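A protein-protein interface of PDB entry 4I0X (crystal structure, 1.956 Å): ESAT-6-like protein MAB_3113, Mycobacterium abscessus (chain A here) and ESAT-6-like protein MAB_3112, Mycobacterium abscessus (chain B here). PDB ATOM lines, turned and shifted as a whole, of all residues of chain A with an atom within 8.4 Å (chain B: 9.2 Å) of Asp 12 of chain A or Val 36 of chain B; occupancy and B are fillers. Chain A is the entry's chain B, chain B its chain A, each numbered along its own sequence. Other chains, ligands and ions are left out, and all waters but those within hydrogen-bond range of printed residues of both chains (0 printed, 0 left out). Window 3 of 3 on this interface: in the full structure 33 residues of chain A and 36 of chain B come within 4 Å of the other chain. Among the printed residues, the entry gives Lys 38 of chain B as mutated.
Asp 12 of chain A touches Val 36 of chain B. His 15 of chain A touches Ser 32 of chain B (CE1 to OG, 3.7 Å). Leu 33 of chain B touches His 15 of chain A. Ile 16 of chain A touches Leu 33 of chain B (N to CD2, 3.9 Å). Trp 37 of chain B touches Ile 16 of chain A. Ile 16 of chain A touches Tyr 45 of chain B. CG2 of Val 30 of chain B touches CG1 of Val 19 of chain A (3.7 Å). Leu 33 of chain B touches Val 19 of chain A. Val 19 of chain A touches Tyr 45 of chain B. CZ2 of Trp 37 of chain B touches CB of Ala 86 of chain A, 3.8 Å away.
Asp 12 of chain A touches just one residue of chain B: Val 36 (3.5 Å). Of the printed residues of chain B, His 15 of chain A touches Ser 32 (3.7 Å) and Leu 33 (3.5 Å). Printed residues of chain B within 4 Å of Ala 86 of chain A: Trp 37. His 87 of chain A touches none of the printed residues of chain B. Gln 31 of chain B touches none of the printed residues of chain A. Printed residues of chain A within 4 Å of Ser 32 of chain B: His 15. Val 36 of chain B touches one residue of chain A. Of the printed residues of chain A, Trp 37 of chain B touches Ile 16 and Ala 86. Printed residues of chain A within 4 Å of Tyr 45 of chain B: Ile 16 and Val 19.
Printed residues of chain B that touch a printed residue of chain A: Val 30, Ser 32, Leu 33, Val 36, Trp 37 and Tyr 45. Hydrophobic or aromatic side chains of chain A that line the printed part of chain B: His 15, Ile 16, Val 19 and Ala 86. Among the printed residues, no Asp or Glu carboxylate lies within 4 Å of a Lys or Arg side-chain nitrogen of the other chain.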
ATOM      1  N   PHE A   9      33.134  -9.819  -5.930  1.00  0.00           N
ATOM      2  CA  PHE A   9      31.992 -10.142  -5.063  1.00  0.00           C
ATOM      3  C   PHE A   9      32.088 -11.614  -4.667  1.00  0.00           C
ATOM      4  O   PHE A   9      31.724 -12.527  -5.426  1.00  0.00           O
ATOM      5  CB  PHE A   9      30.670  -9.890  -5.794  1.00  0.00           C
ATOM      6  CG  PHE A   9      29.477  -9.653  -4.870  1.00  0.00           C
ATOM      7  CD1 PHE A   9      28.716 -10.722  -4.392  1.00  0.00           C
ATOM      8  CD2 PHE A   9      29.099  -8.358  -4.521  1.00  0.00           C
ATOM      9  CE1 PHE A   9      27.608 -10.500  -3.582  1.00  0.00           C
ATOM     10  CE2 PHE A   9      28.005  -8.130  -3.711  1.00  0.00           C
ATOM     11  CZ  PHE A   9      27.258  -9.204  -3.236  1.00  0.00           C
ATOM     12  N   SER A  10      32.626 -11.833  -3.488  1.00  0.00           N
ATOM     13  CA  SER A  10      33.010 -13.151  -3.092  1.00  0.00           C
ATOM     14  C   SER A  10      31.820 -14.117  -2.909  1.00  0.00           C
ATOM     15  O   SER A  10      30.629 -13.729  -2.789  1.00  0.00           O
ATOM     16  CB  SER A  10      33.800 -13.029  -1.814  1.00  0.00           C
ATOM     17  OG  SER A  10      33.027 -12.384  -0.839  1.00  0.00           O
ATOM     18  N   PHE A  11      32.159 -15.392  -2.882  1.00  0.00           N
ATOM     19  CA  PHE A  11      31.180 -16.424  -2.615  1.00  0.00           C
ATOM     20  C   PHE A  11      30.428 -16.118  -1.314  1.00  0.00           C
ATOM     21  O   PHE A  11      29.208 -16.273  -1.232  1.00  0.00           O
ATOM     22  CB  PHE A  11      31.880 -17.769  -2.529  1.00  0.00           C
ATOM     23  CG  PHE A  11      30.955 -18.923  -2.217  1.00  0.00           C
ATOM     24  CD1 PHE A  11      30.630 -19.218  -0.917  1.00  0.00           C
ATOM     25  CD2 PHE A  11      30.412 -19.690  -3.224  1.00  0.00           C
ATOM     26  CE1 PHE A  11      29.767 -20.278  -0.619  1.00  0.00           C
ATOM     27  CE2 PHE A  11      29.557 -20.752  -2.938  1.00  0.00           C
ATOM     28  CZ  PHE A  11      29.242 -21.044  -1.641  1.00  0.00           C
ATOM     29  N   ASP A  12      31.167 -15.688  -0.291  1.00  0.00           N
ATOM     30  CA  ASP A  12      30.581 -15.450   1.031  1.00  0.00           C
ATOM     31  C   ASP A  12      29.519 -14.379   0.981  1.00  0.00           C
ATOM     32  O   ASP A  12      28.481 -14.521   1.589  1.00  0.00           O
ATOM     33  CB  ASP A  12      31.651 -15.090   2.056  1.00  0.00           C
ATOM     34  CG  ASP A  12      32.542 -16.243   2.351  1.00  0.00           C
ATOM     35  OD1 ASP A  12      32.048 -17.376   2.248  1.00  0.00           O
ATOM     36  OD2 ASP A  12      33.725 -16.034   2.661  1.00  0.00           O
ATOM     37  N   LEU A  13      29.735 -13.335   0.189  1.00  0.00           N
ATOM     38  CA  LEU A  13      28.713 -12.293   0.082  1.00  0.00           C
ATOM     39  C   LEU A  13      27.494 -12.809  -0.669  1.00  0.00           C
ATOM     40  O   LEU A  13      26.387 -12.470  -0.320  1.00  0.00           O
ATOM     41  CB  LEU A  13      29.278 -11.055  -0.606  1.00  0.00           C
ATOM     42  CG  LEU A  13      30.436 -10.421   0.166  1.00  0.00           C
ATOM     43  CD1 LEU A  13      31.096  -9.283  -0.635  1.00  0.00           C
ATOM     44  CD2 LEU A  13      29.934  -9.906   1.416  1.00  0.00           C
ATOM     45  N   ASP A  14      27.696 -13.617  -1.707  1.00  0.00           N
ATOM     46  CA  ASP A  14      26.562 -14.253  -2.377  1.00  0.00           C
ATOM     47  C   ASP A  14      25.790 -15.196  -1.434  1.00  0.00           C
ATOM     48  O   ASP A  14      24.566 -15.265  -1.479  1.00  0.00           O
ATOM     49  CB  ASP A  14      26.990 -14.960  -3.652  1.00  0.00           C
ATOM     50  CG  ASP A  14      27.143 -13.996  -4.818  1.00  0.00           C
ATOM     51  OD1 ASP A  14      26.558 -12.895  -4.743  1.00  0.00           O
ATOM     52  OD2 ASP A  14      27.876 -14.313  -5.785  1.00  0.00           O
ATOM     53  N   HIS A  15      26.505 -15.894  -0.560  1.00  0.00           N
ATOM     54  CA  HIS A  15      25.881 -16.766   0.413  1.00  0.00           C
ATOM     55  C   HIS A  15      24.993 -15.953   1.387  1.00  0.00           C
ATOM     56  O   HIS A  15      23.832 -16.286   1.629  1.00  0.00           O
ATOM     57  CB  HIS A  15      26.944 -17.542   1.170  1.00  0.00           C
ATOM     58  CG  HIS A  15      26.387 -18.660   1.967  1.00  0.00           C
ATOM     59  ND1 HIS A  15      27.100 -19.300   2.955  1.00  0.00           N
ATOM     60  CD2 HIS A  15      25.159 -19.228   1.960  1.00  0.00           C
ATOM     61  CE1 HIS A  15      26.348 -20.243   3.494  1.00  0.00           C
ATOM     62  NE2 HIS A  15      25.157 -20.203   2.924  1.00  0.00           N
ATOM     63  N   ILE A  16      25.518 -14.841   1.880  1.00  0.00           N
ATOM     64  CA  ILE A  16      24.746 -13.951   2.759  1.00  0.00           C
ATOM     65  C   ILE A  16      23.475 -13.490   2.068  1.00  0.00           C
ATOM     66  O   ILE A  16      22.396 -13.511   2.644  1.00  0.00           O
ATOM     67  CB  ILE A  16      25.595 -12.711   3.160  1.00  0.00           C
ATOM     68  CG1 ILE A  16      26.767 -13.162   4.015  1.00  0.00           C
ATOM     69  CG2 ILE A  16      24.726 -11.673   3.898  1.00  0.00           C
ATOM     70  CD1 ILE A  16      27.843 -12.195   4.175  1.00  0.00           C
ATOM     71  N   GLU A  17      23.624 -13.037   0.830  1.00  0.00           N
ATOM     72  CA  GLU A  17      22.499 -12.568   0.060  1.00  0.00           C
ATOM     73  C   GLU A  17      21.438 -13.663  -0.159  1.00  0.00           C
ATOM     74  O   GLU A  17      20.243 -13.379  -0.047  1.00  0.00           O
ATOM     75  CB  GLU A  17      22.931 -11.961  -1.270  1.00  0.00           C
ATOM     76  CG  GLU A  17      21.750 -11.489  -2.117  1.00  0.00           C
ATOM     77  CD  GLU A  17      20.881 -10.443  -1.384  1.00  0.00           C
ATOM     78  OE1 GLU A  17      21.412  -9.726  -0.493  1.00  0.00           O
ATOM     79  OE2 GLU A  17      19.667 -10.352  -1.686  1.00  0.00           O
ATOM     80  N   GLN A  18      21.863 -14.897  -0.435  1.00  0.00           N
ATOM     81  CA  GLN A  18      20.933 -16.028  -0.570  1.00  0.00           C
ATOM     82  C   GLN A  18      20.163 -16.355   0.731  1.00  0.00           C
ATOM     83  O   GLN A  18      18.979 -16.615   0.688  1.00  0.00           O
ATOM     84  CB  GLN A  18      21.665 -17.277  -1.132  1.00  0.00           C
ATOM     85  CG  GLN A  18      20.866 -18.561  -1.162  1.00  0.00           C
ATOM     86  CD  GLN A  18      19.519 -18.473  -1.893  1.00  0.00           C
ATOM     87  OE1 GLN A  18      18.582 -19.239  -1.590  1.00  0.00           O
ATOM     88  NE2 GLN A  18      19.432 -17.580  -2.885  1.00  0.00           N
ATOM     89  N   VAL A  19      20.842 -16.338   1.872  1.00  0.00           N
ATOM     90  CA  VAL A  19      20.202 -16.606   3.144  1.00  0.00           C
ATOM     91  C   VAL A  19      19.200 -15.491   3.435  1.00  0.00           C
ATOM     92  O   VAL A  19      18.094 -15.733   3.916  1.00  0.00           O
ATOM     93  CB  VAL A  19      21.247 -16.712   4.290  1.00  0.00           C
ATOM     94  CG1 VAL A  19      20.542 -16.816   5.641  1.00  0.00           C
ATOM     95  CG2 VAL A  19      22.182 -17.861   4.031  1.00  0.00           C
ATOM     96  N   ALA A  86      27.425  -5.078   4.040  1.00  0.00           N
ATOM     97  CA  ALA A  86      28.468  -6.005   3.640  1.00  0.00           C
ATOM     98  C   ALA A  86      28.771  -5.899   2.129  1.00  0.00           C
ATOM     99  O   ALA A  86      29.930  -6.036   1.758  1.00  0.00           O
ATOM    100  CB  ALA A  86      28.105  -7.436   4.030  1.00  0.00           C
ATOM    101  N   HIS A  87      27.750  -5.618   1.298  1.00  0.00           N
ATOM    102  CA  HIS A  87      27.881  -5.536  -0.174  1.00  0.00           C
ATOM    103  C   HIS A  87      28.435  -4.194  -0.658  1.00  0.00           C
ATOM    104  O   HIS A  87      28.626  -4.021  -1.843  1.00  0.00           O
ATOM    105  CB  HIS A  87      26.516  -5.695  -0.895  1.00  0.00           C
ATOM    106  CG  HIS A  87      25.815  -6.989  -0.637  1.00  0.00           C
ATOM    107  ND1 HIS A  87      26.455  -8.210  -0.677  1.00  0.00           N
ATOM    108  CD2 HIS A  87      24.518  -7.256  -0.354  1.00  0.00           C
ATOM    109  CE1 HIS A  87      25.589  -9.172  -0.410  1.00  0.00           C
ATOM    110  NE2 HIS A  87      24.404  -8.620  -0.212  1.00  0.00           N
ATOM    111  N   VAL B  30      21.494 -19.172   8.831  1.00  0.00           N
ATOM    112  CA  VAL B  30      22.038 -17.938   9.363  1.00  0.00           C
ATOM    113  C   VAL B  30      23.263 -18.200  10.174  1.00  0.00           C
ATOM    114  O   VAL B  30      24.273 -17.543   9.965  1.00  0.00           O
ATOM    115  CB  VAL B  30      21.036 -17.154  10.207  1.00  0.00           C
ATOM    116  CG1 VAL B  30      21.763 -16.007  10.922  1.00  0.00           C
ATOM    117  CG2 VAL B  30      19.910 -16.618   9.326  1.00  0.00           C
ATOM    118  N   GLN B  31      23.179 -19.126  11.128  1.00  0.00           N
ATOM    119  CA  GLN B  31      24.349 -19.460  11.934  1.00  0.00           C
ATOM    120  C   GLN B  31      25.537 -19.893  11.064  1.00  0.00           C
ATOM    121  O   GLN B  31      26.670 -19.620  11.419  1.00  0.00           O
ATOM    122  CB  GLN B  31      24.052 -20.571  12.949  1.00  0.00           C
ATOM    123  CG  GLN B  31      22.970 -20.209  13.963  1.00  0.00           C
ATOM    124  CD  GLN B  31      23.122 -18.797  14.530  1.00  0.00           C
ATOM    125  OE1 GLN B  31      24.228 -18.349  14.875  1.00  0.00           O
ATOM    126  NE2 GLN B  31      22.000 -18.090  14.635  1.00  0.00           N
ATOM    127  N   SER B  32      25.297 -20.561   9.935  1.00  0.00           N
ATOM    128  CA  SER B  32      26.439 -21.029   9.133  1.00  0.00           C
ATOM    129  C   SER B  32      27.217 -19.841   8.549  1.00  0.00           C
ATOM    130  O   SER B  32      28.387 -19.997   8.165  1.00  0.00           O
ATOM    131  CB  SER B  32      25.996 -21.969   8.002  1.00  0.00           C
ATOM    132  OG  SER B  32      25.393 -21.225   6.946  1.00  0.00           O
ATOM    133  N   LEU B  33      26.582 -18.672   8.445  1.00  0.00           N
ATOM    134  CA  LEU B  33      27.296 -17.529   7.841  1.00  0.00           C
ATOM    135  C   LEU B  33      28.430 -16.996   8.717  1.00  0.00           C
ATOM    136  O   LEU B  33      29.368 -16.385   8.212  1.00  0.00           O
ATOM    137  CB  LEU B  33      26.350 -16.381   7.553  1.00  0.00           C
ATOM    138  CG  LEU B  33      25.253 -16.658   6.544  1.00  0.00           C
ATOM    139  CD1 LEU B  33      24.351 -15.447   6.603  1.00  0.00           C
ATOM    140  CD2 LEU B  33      25.817 -16.914   5.129  1.00  0.00           C
ATOM    141  N   PHE B  34      28.349 -17.232  10.025  1.00  0.00           N
ATOM    142  CA  PHE B  34      29.221 -16.547  10.970  1.00  0.00           C
ATOM    143  C   PHE B  34      30.575 -17.186  11.116  1.00  0.00           C
ATOM    144  O   PHE B  34      31.493 -16.577  11.664  1.00  0.00           O
ATOM    145  CB  PHE B  34      28.522 -16.389  12.324  1.00  0.00           C
ATOM    146  CG  PHE B  34      27.275 -15.583  12.234  1.00  0.00           C
ATOM    147  CD1 PHE B  34      27.242 -14.440  11.466  1.00  0.00           C
ATOM    148  CD2 PHE B  34      26.115 -15.984  12.871  1.00  0.00           C
ATOM    149  CE1 PHE B  34      26.091 -13.695  11.380  1.00  0.00           C
ATOM    150  CE2 PHE B  34      24.950 -15.241  12.751  1.00  0.00           C
ATOM    151  CZ  PHE B  34      24.942 -14.113  12.021  1.00  0.00           C
ATOM    152  N   GLY B  35      30.713 -18.396  10.571  1.00  0.00           N
ATOM    153  CA  GLY B  35      31.998 -19.030  10.438  1.00  0.00           C
ATOM    154  C   GLY B  35      32.961 -18.214   9.603  1.00  0.00           C
ATOM    155  O   GLY B  35      34.172 -18.196   9.887  1.00  0.00           O
ATOM    156  N   VAL B  36      32.457 -17.502   8.596  1.00  0.00           N
ATOM    157  CA  VAL B  36      33.340 -16.651   7.791  1.00  0.00           C
ATOM    158  C   VAL B  36      33.046 -15.163   7.923  1.00  0.00           C
ATOM    159  O   VAL B  36      33.959 -14.331   7.845  1.00  0.00           O
ATOM    160  CB  VAL B  36      33.294 -16.975   6.290  1.00  0.00           C
ATOM    161  CG1 VAL B  36      33.806 -18.404   6.017  1.00  0.00           C
ATOM    162  CG2 VAL B  36      31.898 -16.744   5.753  1.00  0.00           C
ATOM    163  N   TRP B  37      31.792 -14.814   8.114  1.00  0.00           N
ATOM    164  CA  TRP B  37      31.426 -13.398   8.132  1.00  0.00           C
ATOM    165  C   TRP B  37      31.620 -12.823   9.519  1.00  0.00           C
ATOM    166  O   TRP B  37      30.968 -13.259  10.468  1.00  0.00           O
ATOM    167  CB  TRP B  37      30.008 -13.249   7.652  1.00  0.00           C
ATOM    168  CG  TRP B  37      29.534 -11.861   7.439  1.00  0.00           C
ATOM    169  CD1 TRP B  37      30.290 -10.719   7.202  1.00  0.00           C
ATOM    170  CD2 TRP B  37      28.170 -11.446   7.445  1.00  0.00           C
ATOM    171  NE1 TRP B  37      29.467  -9.644   7.020  1.00  0.00           N
ATOM    172  CE2 TRP B  37      28.157 -10.052   7.162  1.00  0.00           C
ATOM    173  CE3 TRP B  37      26.954 -12.122   7.620  1.00  0.00           C
ATOM    174  CZ2 TRP B  37      26.987  -9.332   7.070  1.00  0.00           C
ATOM    175  CZ3 TRP B  37      25.769 -11.403   7.527  1.00  0.00           C
ATOM    176  CH2 TRP B  37      25.787 -10.016   7.250  1.00  0.00           C
ATOM    177  N   LYS B  38      32.553 -11.867   9.611  1.00  0.00           N
ATOM    178  CA  LYS B  38      32.915 -11.192  10.856  1.00  0.00           C
ATOM    179  C   LYS B  38      32.732  -9.655  10.744  1.00  0.00           C
ATOM    180  O   LYS B  38      32.664  -9.105   9.655  1.00  0.00           O
ATOM    181  CB  LYS B  38      34.382 -11.466  11.212  1.00  0.00           C
ATOM    182  CG  LYS B  38      34.837 -12.911  11.043  1.00  0.00           C
ATOM    183  CD  LYS B  38      34.050 -13.848  11.957  1.00  0.00           C
ATOM    184  CE  LYS B  38      34.564 -15.294  11.899  1.00  0.00           C
ATOM    185  NZ  LYS B  38      34.052 -16.088  13.066  1.00  0.00           N
ATOM    186  N   GLY B  39      32.668  -8.974  11.877  1.00  0.00           N
ATOM    187  CA  GLY B  39      32.601  -7.527  11.897  1.00  0.00           C
ATOM    188  C   GLY B  39      31.236  -6.970  12.264  1.00  0.00           C
ATOM    189  O   GLY B  39      30.286  -7.709  12.591  1.00  0.00           O
ATOM    190  N   ALA B  42      28.130  -8.246  10.348  1.00  0.00           N
ATOM    191  CA  ALA B  42      27.785  -9.587  10.788  1.00  0.00           C
ATOM    192  C   ALA B  42      27.063  -9.542  12.130  1.00  0.00           C
ATOM    193  O   ALA B  42      26.094 -10.273  12.346  1.00  0.00           O
ATOM    194  CB  ALA B  42      29.006 -10.436  10.832  1.00  0.00           C
ATOM    195  N   TYR B  45      23.534  -8.324  11.719  1.00  0.00           N
ATOM    196  CA  TYR B  45      22.753  -9.393  11.112  1.00  0.00           C
ATOM    197  C   TYR B  45      22.342 -10.440  12.150  1.00  0.00           C
ATOM    198  O   TYR B  45      21.194 -10.858  12.221  1.00  0.00           O
ATOM    199  CB  TYR B  45      23.579 -10.052  10.016  1.00  0.00           C
ATOM    200  CG  TYR B  45      22.775 -10.887   9.031  1.00  0.00           C
ATOM    201  CD1 TYR B  45      22.542 -12.225   9.259  1.00  0.00           C
ATOM    202  CD2 TYR B  45      22.326 -10.344   7.850  1.00  0.00           C
ATOM    203  CE1 TYR B  45      21.867 -12.997   8.344  1.00  0.00           C
ATOM    204  CE2 TYR B  45      21.626 -11.092   6.950  1.00  0.00           C
ATOM    205  CZ  TYR B  45      21.412 -12.438   7.191  1.00  0.00           C
ATOM    206  OH  TYR B  45      20.732 -13.202   6.251  1.00  0.00           O
ATOM    207  N   ARG B  46      23.303 -10.884  12.945  1.00  0.00           N
ATOM    208  CA  ARG B  46      23.001 -11.779  14.045  1.00  0.00           C
ATOM    209  C   ARG B  46      21.901 -11.253  14.977  1.00  0.00           C
ATOM    210  O   ARG B  46      21.042 -12.006  15.370  1.00  0.00           O
ATOM    211  CB  ARG B  46      24.258 -12.102  14.845  1.00  0.00           C
ATOM    212  CG  ARG B  46      23.981 -13.062  15.991  1.00  0.00           C
ATOM    213  CD  ARG B  46      25.176 -13.208  16.896  1.00  0.00           C
ATOM    214  NE  ARG B  46      26.391 -13.599  16.198  1.00  0.00           N
ATOM    215  CZ  ARG B  46      26.892 -14.837  16.162  1.00  0.00           C
ATOM    216  NH1 ARG B  46      26.270 -15.850  16.768  1.00  0.00           N
ATOM    217  NH2 ARG B  46      28.036 -15.066  15.511  1.00  0.00           N
